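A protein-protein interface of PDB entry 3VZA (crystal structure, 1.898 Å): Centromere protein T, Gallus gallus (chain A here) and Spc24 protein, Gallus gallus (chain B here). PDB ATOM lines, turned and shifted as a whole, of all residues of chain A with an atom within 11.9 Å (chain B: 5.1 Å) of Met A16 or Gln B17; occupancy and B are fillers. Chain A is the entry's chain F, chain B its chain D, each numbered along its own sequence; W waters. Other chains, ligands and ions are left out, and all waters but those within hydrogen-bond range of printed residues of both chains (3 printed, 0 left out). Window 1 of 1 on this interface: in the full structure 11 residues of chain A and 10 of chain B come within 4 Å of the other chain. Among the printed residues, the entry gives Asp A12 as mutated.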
ATOM      1  N   ALA A   4      27.676   4.406  44.188  1.00  0.00           N
ATOM      2  CA  ALA A   4      26.804   3.419  43.560  1.00  0.00           C
ATOM      3  C   ALA A   4      27.001   3.248  42.039  1.00  0.00           C
ATOM      4  O   ALA A   4      26.560   2.242  41.483  1.00  0.00           O
ATOM      5  CB  ALA A   4      25.332   3.729  43.878  1.00  0.00           C
ATOM      6  N   PHE A   5      27.615   4.234  41.375  1.00  0.00           N
ATOM      7  CA  PHE A   5      27.806   4.202  39.911  1.00  0.00           C
ATOM      8  C   PHE A   5      29.184   3.718  39.576  1.00  0.00           C
ATOM      9  O   PHE A   5      29.624   3.784  38.432  1.00  0.00           O
ATOM     10  CB  PHE A   5      27.391   5.558  39.235  1.00  0.00           C
ATOM     11  CG  PHE A   5      25.917   5.818  39.373  1.00  0.00           C
ATOM     12  CD1 PHE A   5      25.022   5.186  38.557  1.00  0.00           C
ATOM     13  CD2 PHE A   5      25.431   6.601  40.394  1.00  0.00           C
ATOM     14  CE1 PHE A   5      23.652   5.372  38.731  1.00  0.00           C
ATOM     15  CE2 PHE A   5      24.074   6.800  40.567  1.00  0.00           C
ATOM     16  CZ  PHE A   5      23.188   6.199  39.752  1.00  0.00           C
ATOM     17  N   SER A   6      29.899   3.238  40.598  1.00  0.00           N
ATOM     18  CA  SER A   6      31.276   2.929  40.374  1.00  0.00           C
ATOM     19  C   SER A   6      31.463   2.025  39.114  1.00  0.00           C
ATOM     20  O   SER A   6      32.360   2.211  38.252  1.00  0.00           O
ATOM     21  CB  SER A   6      31.796   2.267  41.637  1.00  0.00           C
ATOM     22  OG  SER A   6      33.190   2.246  41.585  1.00  0.00           O
ATOM     23  N   GLU A   7      30.626   1.026  39.060  1.00  0.00           N
ATOM     24  CA  GLU A   7      30.794   0.029  38.015  1.00  0.00           C
ATOM     25  C   GLU A   7      30.460   0.613  36.644  1.00  0.00           C
ATOM     26  O   GLU A   7      31.240   0.492  35.683  1.00  0.00           O
ATOM     27  CB  GLU A   7      29.836  -1.137  38.243  1.00  0.00           C
ATOM     28  CG  GLU A   7      30.068  -2.100  37.059  1.00  0.00           C
ATOM     29  CD  GLU A   7      29.270  -3.420  37.206  1.00  0.00           C
ATOM     30  OE1 GLU A   7      28.495  -3.562  38.137  1.00  0.00           O
ATOM     31  OE2 GLU A   7      29.434  -4.291  36.351  1.00  0.00           O
ATOM     32  N   LEU A   8      29.322   1.279  36.572  1.00  0.00           N
ATOM     33  CA  LEU A   8      29.045   2.025  35.308  1.00  0.00           C
ATOM     34  C   LEU A   8      30.103   3.057  34.926  1.00  0.00           C
ATOM     35  O   LEU A   8      30.468   3.134  33.743  1.00  0.00           O
ATOM     36  CB  LEU A   8      27.641   2.645  35.320  1.00  0.00           C
ATOM     37  CG  LEU A   8      26.417   1.721  35.384  1.00  0.00           C
ATOM     38  CD1 LEU A   8      25.073   2.454  35.223  1.00  0.00           C
ATOM     39  CD2 LEU A   8      26.561   0.683  34.261  1.00  0.00           C
ATOM     40  N   ASP A   9      30.609   3.872  35.876  1.00  0.00           N
ATOM     41  CA  ASP A   9      31.685   4.779  35.512  1.00  0.00           C
ATOM     42  C   ASP A   9      32.927   4.178  34.933  1.00  0.00           C
ATOM     43  O   ASP A   9      33.574   4.763  34.065  1.00  0.00           O
ATOM     44  CB  ASP A   9      32.112   5.690  36.720  1.00  0.00           C
ATOM     45  CG  ASP A   9      30.953   6.493  37.289  1.00  0.00           C
ATOM     46  OD1 ASP A   9      29.984   6.764  36.547  1.00  0.00           O
ATOM     47  OD2 ASP A   9      30.974   6.860  38.499  1.00  0.00           O
ATOM     48  N   SER A  10      33.319   2.999  35.422  1.00  0.00           N
ATOM     49  CA  SER A  10      34.432   2.391  34.763  1.00  0.00           C
ATOM     50  C   SER A  10      34.171   1.431  33.548  1.00  0.00           C
ATOM     51  O   SER A  10      35.113   1.071  32.848  1.00  0.00           O
ATOM     52  CB  SER A  10      35.335   1.653  35.777  1.00  0.00           C
ATOM     53  OG  SER A  10      34.656   0.499  36.180  1.00  0.00           O
ATOM     54  N   ALA A  11      32.935   1.075  33.279  1.00  0.00           N
ATOM     55  CA  ALA A  11      32.647   0.213  32.109  1.00  0.00           C
ATOM     56  C   ALA A  11      33.030   0.849  30.798  1.00  0.00           C
ATOM     57  O   ALA A  11      33.032   2.067  30.641  1.00  0.00           O
ATOM     58  CB  ALA A  11      31.136  -0.126  32.125  1.00  0.00           C
ATOM     59  N   ASP A  12      33.399   0.029  29.837  1.00  0.00           N
ATOM     60  CA  ASP A  12      33.825   0.524  28.554  1.00  0.00           C
ATOM     61  C   ASP A  12      32.496   0.729  27.778  1.00  0.00           C
ATOM     62  O   ASP A  12      31.607  -0.145  27.824  1.00  0.00           O
ATOM     63  CB  ASP A  12      34.737  -0.464  27.889  1.00  0.00           C
ATOM     64  CG  ASP A  12      35.257   0.059  26.605  1.00  0.00           C
ATOM     65  OD1 ASP A  12      36.428   0.404  26.559  1.00  0.00           O
ATOM     66  OD2 ASP A  12      34.506   0.164  25.582  1.00  0.00           O
ATOM     67  N   PRO A  13      32.308   1.920  27.125  1.00  0.00           N
ATOM     68  CA  PRO A  13      31.023   2.142  26.446  1.00  0.00           C
ATOM     69  C   PRO A  13      30.771   1.073  25.358  1.00  0.00           C
ATOM     70  O   PRO A  13      29.609   0.825  25.121  1.00  0.00           O
ATOM     71  CB  PRO A  13      31.265   3.497  25.743  1.00  0.00           C
ATOM     72  CG  PRO A  13      32.138   4.278  26.788  1.00  0.00           C
ATOM     73  CD  PRO A  13      33.169   3.138  27.134  1.00  0.00           C
ATOM     74  N   ARG A  14      31.818   0.533  24.743  1.00  0.00           N
ATOM     75  CA  ARG A  14      31.618  -0.499  23.708  1.00  0.00           C
ATOM     76  C   ARG A  14      30.939  -1.787  24.259  1.00  0.00           C
ATOM     77  O   ARG A  14      30.140  -2.442  23.572  1.00  0.00           O
ATOM     78  CB  ARG A  14      32.937  -0.853  23.048  1.00  0.00           C
ATOM     79  CG  ARG A  14      33.530   0.306  22.213  1.00  0.00           C
ATOM     80  CD  ARG A  14      34.939  -0.085  21.808  1.00  0.00           C
ATOM     81  NE  ARG A  14      35.850   0.030  22.940  1.00  0.00           N
ATOM     82  CZ  ARG A  14      37.141  -0.184  22.839  1.00  0.00           C
ATOM     83  NH1 ARG A  14      37.661  -0.517  21.672  1.00  0.00           N
ATOM     84  NH2 ARG A  14      37.913  -0.028  23.917  1.00  0.00           N
ATOM     85  N   VAL A  15      31.355  -2.190  25.445  1.00  0.00           N
ATOM     86  CA  VAL A  15      30.631  -3.219  26.191  1.00  0.00           C
ATOM     87  C   VAL A  15      29.217  -2.845  26.441  1.00  0.00           C
ATOM     88  O   VAL A  15      28.317  -3.665  26.187  1.00  0.00           O
ATOM     89  CB  VAL A  15      31.349  -3.614  27.513  1.00  0.00           C
ATOM     90  CG1 VAL A  15      30.472  -4.549  28.350  1.00  0.00           C
ATOM     91  CG2 VAL A  15      32.746  -4.132  27.192  1.00  0.00           C
ATOM     92  N   MET A  16      28.934  -1.620  26.954  1.00  0.00           N
ATOM     93  CA  MET A  16      27.570  -1.257  27.200  1.00  0.00           C
ATOM     94  C   MET A  16      26.710  -1.223  25.899  1.00  0.00           C
ATOM     95  O   MET A  16      25.473  -1.540  25.919  1.00  0.00           O
ATOM     96  CB  MET A  16      27.575   0.152  27.876  1.00  0.00           C
ATOM     97  CG  MET A  16      28.326   0.106  29.189  1.00  0.00           C
ATOM     98  SD  MET A  16      28.179   1.761  30.070  1.00  0.00           S
ATOM     99  CE  MET A  16      26.569   1.647  30.636  1.00  0.00           C
ATOM    100  N   LEU A  17      27.333  -0.802  24.810  1.00  0.00           N
ATOM    101  CA  LEU A  17      26.591  -0.684  23.560  1.00  0.00           C
ATOM    102  C   LEU A  17      26.274  -2.100  23.062  1.00  0.00           C
ATOM    103  O   LEU A  17      25.139  -2.428  22.690  1.00  0.00           O
ATOM    104  CB  LEU A  17      27.462   0.022  22.538  1.00  0.00           C
ATOM    105  CG  LEU A  17      27.501   1.569  22.921  1.00  0.00           C
ATOM    106  CD1 LEU A  17      28.655   2.137  22.049  1.00  0.00           C
ATOM    107  CD2 LEU A  17      26.112   2.227  22.546  1.00  0.00           C
ATOM    108  N   ARG A  18      27.281  -2.953  23.139  1.00  0.00           N
ATOM    109  CA  ARG A  18      27.062  -4.361  22.776  1.00  0.00           C
ATOM    110  C   ARG A  18      25.998  -5.021  23.677  1.00  0.00           C
ATOM    111  O   ARG A  18      25.201  -5.865  23.176  1.00  0.00           O
ATOM    112  CB  ARG A  18      28.452  -5.077  22.715  1.00  0.00           C
ATOM    113  CG  ARG A  18      28.478  -6.419  22.143  1.00  0.00           C
ATOM    114  CD  ARG A  18      27.814  -6.516  20.774  1.00  0.00           C
ATOM    115  NE  ARG A  18      28.695  -6.235  19.647  1.00  0.00           N
ATOM    116  CZ  ARG A  18      28.300  -6.385  18.406  1.00  0.00           C
ATOM    117  NH1 ARG A  18      27.076  -6.879  18.159  1.00  0.00           N
ATOM    118  NH2 ARG A  18      29.115  -6.138  17.441  1.00  0.00           N
ATOM    119  N   ARG A  19      25.894  -4.685  24.967  1.00  0.00           N
ATOM    120  CA  ARG A  19      24.831  -5.246  25.807  1.00  0.00           C
ATOM    121  C   ARG A  19      23.442  -4.931  25.235  1.00  0.00           C
ATOM    122  O   ARG A  19      22.500  -5.771  25.266  1.00  0.00           O
ATOM    123  CB  ARG A  19      24.835  -4.768  27.249  1.00  0.00           C
ATOM    124  CG  ARG A  19      26.051  -5.119  28.062  1.00  0.00           C
ATOM    125  CD  ARG A  19      25.957  -6.571  28.398  1.00  0.00           C
ATOM    126  NE  ARG A  19      26.717  -6.925  29.599  1.00  0.00           N
ATOM    127  CZ  ARG A  19      27.073  -8.180  29.850  1.00  0.00           C
ATOM    128  NH1 ARG A  19      26.693  -9.128  28.973  1.00  0.00           N
ATOM    129  NH2 ARG A  19      27.753  -8.484  30.967  1.00  0.00           N
ATOM    130  N   ILE A  20      23.267  -3.687  24.798  1.00  0.00           N
ATOM    131  CA  ILE A  20      21.956  -3.364  24.184  1.00  0.00           C
ATOM    132  C   ILE A  20      21.789  -4.143  22.875  1.00  0.00           C
ATOM    133  O   ILE A  20      20.719  -4.700  22.644  1.00  0.00           O
ATOM    134  CB  ILE A  20      21.857  -1.818  23.836  1.00  0.00           C
ATOM    135  CG1 ILE A  20      22.004  -1.064  25.169  1.00  0.00           C
ATOM    136  CG2 ILE A  20      20.462  -1.509  23.276  1.00  0.00           C
ATOM    137  CD1 ILE A  20      22.019   0.523  24.895  1.00  0.00           C
ATOM    138  N   ILE A  21      22.819  -4.199  22.071  1.00  0.00           N
ATOM    139  CA  ILE A  21      22.643  -4.711  20.708  1.00  0.00           C
ATOM    140  C   ILE A  21      22.299  -6.266  20.863  1.00  0.00           C
ATOM    141  O   ILE A  21      21.346  -6.812  20.276  1.00  0.00           O
ATOM    142  CB  ILE A  21      23.918  -4.543  19.939  1.00  0.00           C
ATOM    143  CG1 ILE A  21      24.178  -3.028  19.538  1.00  0.00           C
ATOM    144  CG2 ILE A  21      23.883  -5.328  18.609  1.00  0.00           C
ATOM    145  CD1 ILE A  21      25.549  -2.793  19.036  1.00  0.00           C
ATOM    146  N   GLN A  22      22.985  -6.938  21.764  1.00  0.00           N
ATOM    147  CA  GLN A  22      22.781  -8.423  21.886  1.00  0.00           C
ATOM    148  C   GLN A  22      21.535  -8.801  22.590  1.00  0.00           C
ATOM    149  O   GLN A  22      21.119  -9.948  22.479  1.00  0.00           O
ATOM    150  CB  GLN A  22      23.986  -9.085  22.642  1.00  0.00           C
ATOM    151  CG  GLN A  22      25.321  -8.802  21.988  1.00  0.00           C
ATOM    152  CD  GLN A  22      25.457  -9.280  20.546  1.00  0.00           C
ATOM    153  OE1 GLN A  22      25.302  -8.517  19.583  1.00  0.00           O
ATOM    154  NE2 GLN A  22      25.798 -10.572  20.375  1.00  0.00           N
ATOM    155  N   ASN A  23      20.998  -7.932  23.464  1.00  0.00           N
ATOM    156  CA  ASN A  23      19.879  -8.324  24.298  1.00  0.00           C
ATOM    157  C   ASN A  23      18.505  -7.731  24.011  1.00  0.00           C
ATOM    158  O   ASN A  23      17.512  -8.084  24.643  1.00  0.00           O
ATOM    159  CB  ASN A  23      20.267  -8.128  25.754  1.00  0.00           C
ATOM    160  CG  ASN A  23      21.462  -8.950  26.109  1.00  0.00           C
ATOM    161  OD1 ASN A  23      21.333 -10.175  26.287  1.00  0.00           O
ATOM    162  ND2 ASN A  23      22.641  -8.310  26.235  1.00  0.00           N
ATOM    163  N   GLN A  24      18.447  -6.814  23.063  1.00  0.00           N
ATOM    164  CA  GLN A  24      17.175  -6.143  22.822  1.00  0.00           C
ATOM    165  C   GLN A  24      16.785  -6.592  21.435  1.00  0.00           C
ATOM    166  O   GLN A  24      17.610  -6.640  20.527  1.00  0.00           O
ATOM    167  CB  GLN A  24      17.336  -4.622  22.799  1.00  0.00           C
ATOM    168  CG  GLN A  24      17.778  -4.037  24.126  1.00  0.00           C
ATOM    169  CD  GLN A  24      16.754  -4.249  25.226  1.00  0.00           C
ATOM    170  OE1 GLN A  24      16.234  -5.283  25.416  1.00  0.00           O
ATOM    171  NE2 GLN A  24      16.481  -3.248  25.947  1.00  0.00           N
ATOM    172  N   ALA B  13      17.015  -2.503  31.142  1.00  0.00           N
ATOM    173  CA  ALA B  13      18.045  -2.032  32.028  1.00  0.00           C
ATOM    174  C   ALA B  13      19.251  -1.547  31.246  1.00  0.00           C
ATOM    175  O   ALA B  13      19.879  -0.562  31.619  1.00  0.00           O
ATOM    176  CB  ALA B  13      18.475  -3.138  32.997  1.00  0.00           C
ATOM    177  N   TYR B  14      19.630  -2.246  30.197  1.00  0.00           N
ATOM    178  CA  TYR B  14      20.841  -1.885  29.481  1.00  0.00           C
ATOM    179  C   TYR B  14      20.734  -0.480  28.827  1.00  0.00           C
ATOM    180  O   TYR B  14      21.792   0.204  28.692  1.00  0.00           O
ATOM    181  CB  TYR B  14      21.152  -2.876  28.391  1.00  0.00           C
ATOM    182  CG  TYR B  14      21.636  -4.253  29.009  1.00  0.00           C
ATOM    183  CD1 TYR B  14      22.560  -4.274  30.079  1.00  0.00           C
ATOM    184  CD2 TYR B  14      21.156  -5.472  28.549  1.00  0.00           C
ATOM    185  CE1 TYR B  14      23.047  -5.465  30.647  1.00  0.00           C
ATOM    186  CE2 TYR B  14      21.612  -6.717  29.140  1.00  0.00           C
ATOM    187  CZ  TYR B  14      22.557  -6.702  30.156  1.00  0.00           C
ATOM    188  OH  TYR B  14      23.091  -7.885  30.698  1.00  0.00           O
ATOM    189  N   VAL B  15      19.580  -0.192  28.269  1.00  0.00           N
ATOM    190  CA  VAL B  15      19.400   1.157  27.683  1.00  0.00           C
ATOM    191  C   VAL B  15      19.467   2.227  28.781  1.00  0.00           C
ATOM    192  O   VAL B  15      20.107   3.274  28.592  1.00  0.00           O
ATOM    193  CB  VAL B  15      18.086   1.273  26.867  1.00  0.00           C
ATOM    194  CG1 VAL B  15      17.932   2.730  26.361  1.00  0.00           C
ATOM    195  CG2 VAL B  15      18.148   0.334  25.715  1.00  0.00           C
ATOM    196  N   THR B  16      18.834   2.004  29.934  1.00  0.00           N
ATOM    197  CA  THR B  16      18.850   3.087  30.930  1.00  0.00           C
ATOM    198  C   THR B  16      20.273   3.222  31.479  1.00  0.00           C
ATOM    199  O   THR B  16      20.747   4.315  31.747  1.00  0.00           O
ATOM    200  CB  THR B  16      17.815   2.880  32.034  1.00  0.00           C
ATOM    201  OG1 THR B  16      17.970   1.581  32.575  1.00  0.00           O
ATOM    202  CG2 THR B  16      16.400   2.977  31.452  1.00  0.00           C
ATOM    203  N   GLN B  17      21.001   2.105  31.554  1.00  0.00           N
ATOM    204  CA  GLN B  17      22.411   2.188  31.965  1.00  0.00           C
ATOM    205  C   GLN B  17      23.226   3.040  30.998  1.00  0.00           C
ATOM    206  O   GLN B  17      24.075   3.860  31.435  1.00  0.00           O
ATOM    207  CB  GLN B  17      23.041   0.753  32.099  1.00  0.00           C
ATOM    208  CG  GLN B  17      22.655   0.041  33.398  1.00  0.00           C
ATOM    209  CD  GLN B  17      22.906  -1.468  33.268  1.00  0.00           C
ATOM    210  OE1 GLN B  17      23.799  -1.891  32.526  1.00  0.00           O
ATOM    211  NE2 GLN B  17      22.081  -2.273  33.938  1.00  0.00           N
ATOM    212  N   LEU B  18      23.008   2.823  29.687  1.00  0.00           N
ATOM    213  CA  LEU B  18      23.704   3.702  28.728  1.00  0.00           C
ATOM    214  C   LEU B  18      23.270   5.184  28.836  1.00  0.00           C
ATOM    215  O   LEU B  18      24.105   6.105  28.627  1.00  0.00           O
ATOM    216  CB  LEU B  18      23.442   3.214  27.293  1.00  0.00           C
ATOM    217  CG  LEU B  18      24.367   3.867  26.259  1.00  0.00           C
ATOM    218  CD1 LEU B  18      25.785   3.201  26.294  1.00  0.00           C
ATOM    219  CD2 LEU B  18      23.715   3.757  24.853  1.00  0.00           C
ATOM    220  N   TYR B  19      22.005   5.453  29.169  1.00  0.00           N
ATOM    221  CA  TYR B  19      21.624   6.884  29.302  1.00  0.00           C
ATOM    222  C   TYR B  19      22.401   7.497  30.463  1.00  0.00           C
ATOM    223  O   TYR B  19      22.745   8.706  30.418  1.00  0.00           O
ATOM    224  CB  TYR B  19      20.131   7.079  29.639  1.00  0.00           C
ATOM    225  CG  TYR B  19      19.178   7.053  28.466  1.00  0.00           C
ATOM    226  CD1 TYR B  19      19.236   8.026  27.484  1.00  0.00           C
ATOM    227  CD2 TYR B  19      18.161   6.104  28.407  1.00  0.00           C
ATOM    228  CE1 TYR B  19      18.362   8.000  26.416  1.00  0.00           C
ATOM    229  CE2 TYR B  19      17.233   6.102  27.321  1.00  0.00           C
ATOM    230  CZ  TYR B  19      17.361   7.062  26.345  1.00  0.00           C
ATOM    231  OH  TYR B  19      16.462   7.094  25.268  1.00  0.00           O
ATOM    232  N   TYR B  20      22.636   6.720  31.526  1.00  0.00           N
ATOM    233  CA  TYR B  20      23.509   7.197  32.606  1.00  0.00           C
ATOM    234  C   TYR B  20      24.924   7.437  32.105  1.00  0.00           C
ATOM    235  O   TYR B  20      25.526   8.445  32.448  1.00  0.00           O
ATOM    236  CB  TYR B  20      23.509   6.264  33.855  1.00  0.00           C
ATOM    237  CG  TYR B  20      24.600   6.672  34.807  1.00  0.00           C
ATOM    238  CD1 TYR B  20      24.390   7.687  35.773  1.00  0.00           C
ATOM    239  CD2 TYR B  20      25.870   6.198  34.660  1.00  0.00           C
ATOM    240  CE1 TYR B  20      25.451   8.103  36.605  1.00  0.00           C
ATOM    241  CE2 TYR B  20      26.914   6.617  35.455  1.00  0.00           C
ATOM    242  CZ  TYR B  20      26.701   7.561  36.430  1.00  0.00           C
ATOM    243  OH  TYR B  20      27.775   7.949  37.176  1.00  0.00           O
ATOM    244  N   LYS B  21      25.470   6.483  31.321  1.00  0.00           N
ATOM    245  CA  LYS B  21      26.850   6.594  30.841  1.00  0.00           C
ATOM    246  C   LYS B  21      26.986   7.913  30.038  1.00  0.00           C
ATOM    247  O   LYS B  21      28.002   8.595  30.102  1.00  0.00           O
ATOM    248  CB  LYS B  21      27.273   5.384  29.966  1.00  0.00           C
ATOM    249  CG  LYS B  21      28.789   5.404  29.619  1.00  0.00           C
ATOM    250  CD  LYS B  21      29.649   5.012  30.870  1.00  0.00           C
ATOM    251  CE  LYS B  21      31.066   4.518  30.492  1.00  0.00           C
ATOM    252  NZ  LYS B  21      31.953   4.509  31.767  1.00  0.00           N
HETATM  253  O   HOH W   1      24.304  -0.629  28.427  1.00  0.00           O
HETATM  254  O   HOH W   2      32.260   7.200  32.408  1.00  0.00           O
HETATM  255  O   HOH W   3      29.406   8.829  39.386  1.00  0.00           O
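O of Arg A19 sits at hydrogen-bond distance from ND2 of Asn A23 (2.7 Å).
Water W1 bridges the backbone carbonyl oxygen (O) of Tyr B14 (2.7 Å) and the backbone carbonyl oxygen (O) of Met A16 (2.9 Å).
Water W3 lies within hydrogen-bond range of the side-chain carboxylate of Asp A9 and the side-chain hydroxyl of Tyr B20.
Water W2 bridges NZ of Lys B21 and O of Asp A9.
Among the printed residues, merely in contact across the chains: Phe A5 with Tyr B20 (3.2 Å), Met A16 with Gln B17 (3.4 Å), Asn A23 with Tyr B14 (3.5 Å), Arg A19 with Tyr B14 (3.6 Å), Ile A20 with Leu B18 (3.7 Å), Met A16 with Lys B21 (3.7 Å), Leu A17 with Leu B18 (3.7 Å), Ile A20 with Tyr B14 (3.8 Å), Ile A20 with Val B15 (3.8 Å), Pro A13 with Lys B21 (3.9 Å), Met A16 with Leu B18 (3.9 Å), Leu A8 with Tyr B20 (3.9 Å), Leu A8 with Gln B17 (3.9 Å) and Gln A24 with Val B15 (3.96 Å).
Hydrophobic or aromatic side chains of chain A that line the printed part of chain B: Phe A5, Leu A8, Pro A13, Met A16, Leu A17 and Ile A20.
Of the 9 printed residues of chain B, 6 touch a printed residue of chain A.
Among the printed residues, 18 pairs touch across the chains.
Among the printed residues, no Asp or Glu carboxylate lies within 4 Å of a Lys or Arg side-chain nitrogen of the other chain.
Of chain B, only Gln B17 (3.4 Å), Leu B18 (3.9 Å) and Lys B21 (3.7 Å) come within 4 Å of Met A16.
Of chain A, only Leu A8 (3.9 Å) and Met A16 (3.4 Å) come within 4 Å of Gln B17.
Printed residues of chain A within 4 Å of Tyr B14: Arg A19 (3.6 Å), Ile A20 (3.8 Å) and Asn A23 (3.5 Å).
Of the printed residues of chain A, Val B15 touches Ile A20 (3.8 Å) and Gln A24 (3.96 Å).
No residue of chain A comes within 4 Å of Thr B16.
Leu B18 touches just these residues of chain A: Met A16, Leu A17 and Ile A20.
Lys B21 touches five residues of chain A.
Printed residues of chain B within 4 Å of Ala A11: Lys B21 (2.9 Å).
Printed residues of chain B within 4 Å of Phe A5: Tyr B20 (3.2 Å).
Ser A6 touches none of the printed residues of chain B.
The nearest residue of chain A that does not touch Gln B17 is Arg A19 (6.0 Å).
NZ of Lys B21 lies within hydrogen-bond range of O of Leu A8, 2.8 Å away.
NZ of Lys B21 lies within hydrogen-bond range of O of Ala A11, 2.9 Å away.
NZ of Lys B21 lies within hydrogen-bond range of O of Asp A9 (2.8 Å).
The side-chain carboxylate (OD1) of Asp A9 lies within hydrogen-bond range of the side-chain hydroxyl (OH) of Tyr B20, at 2.6 Å.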
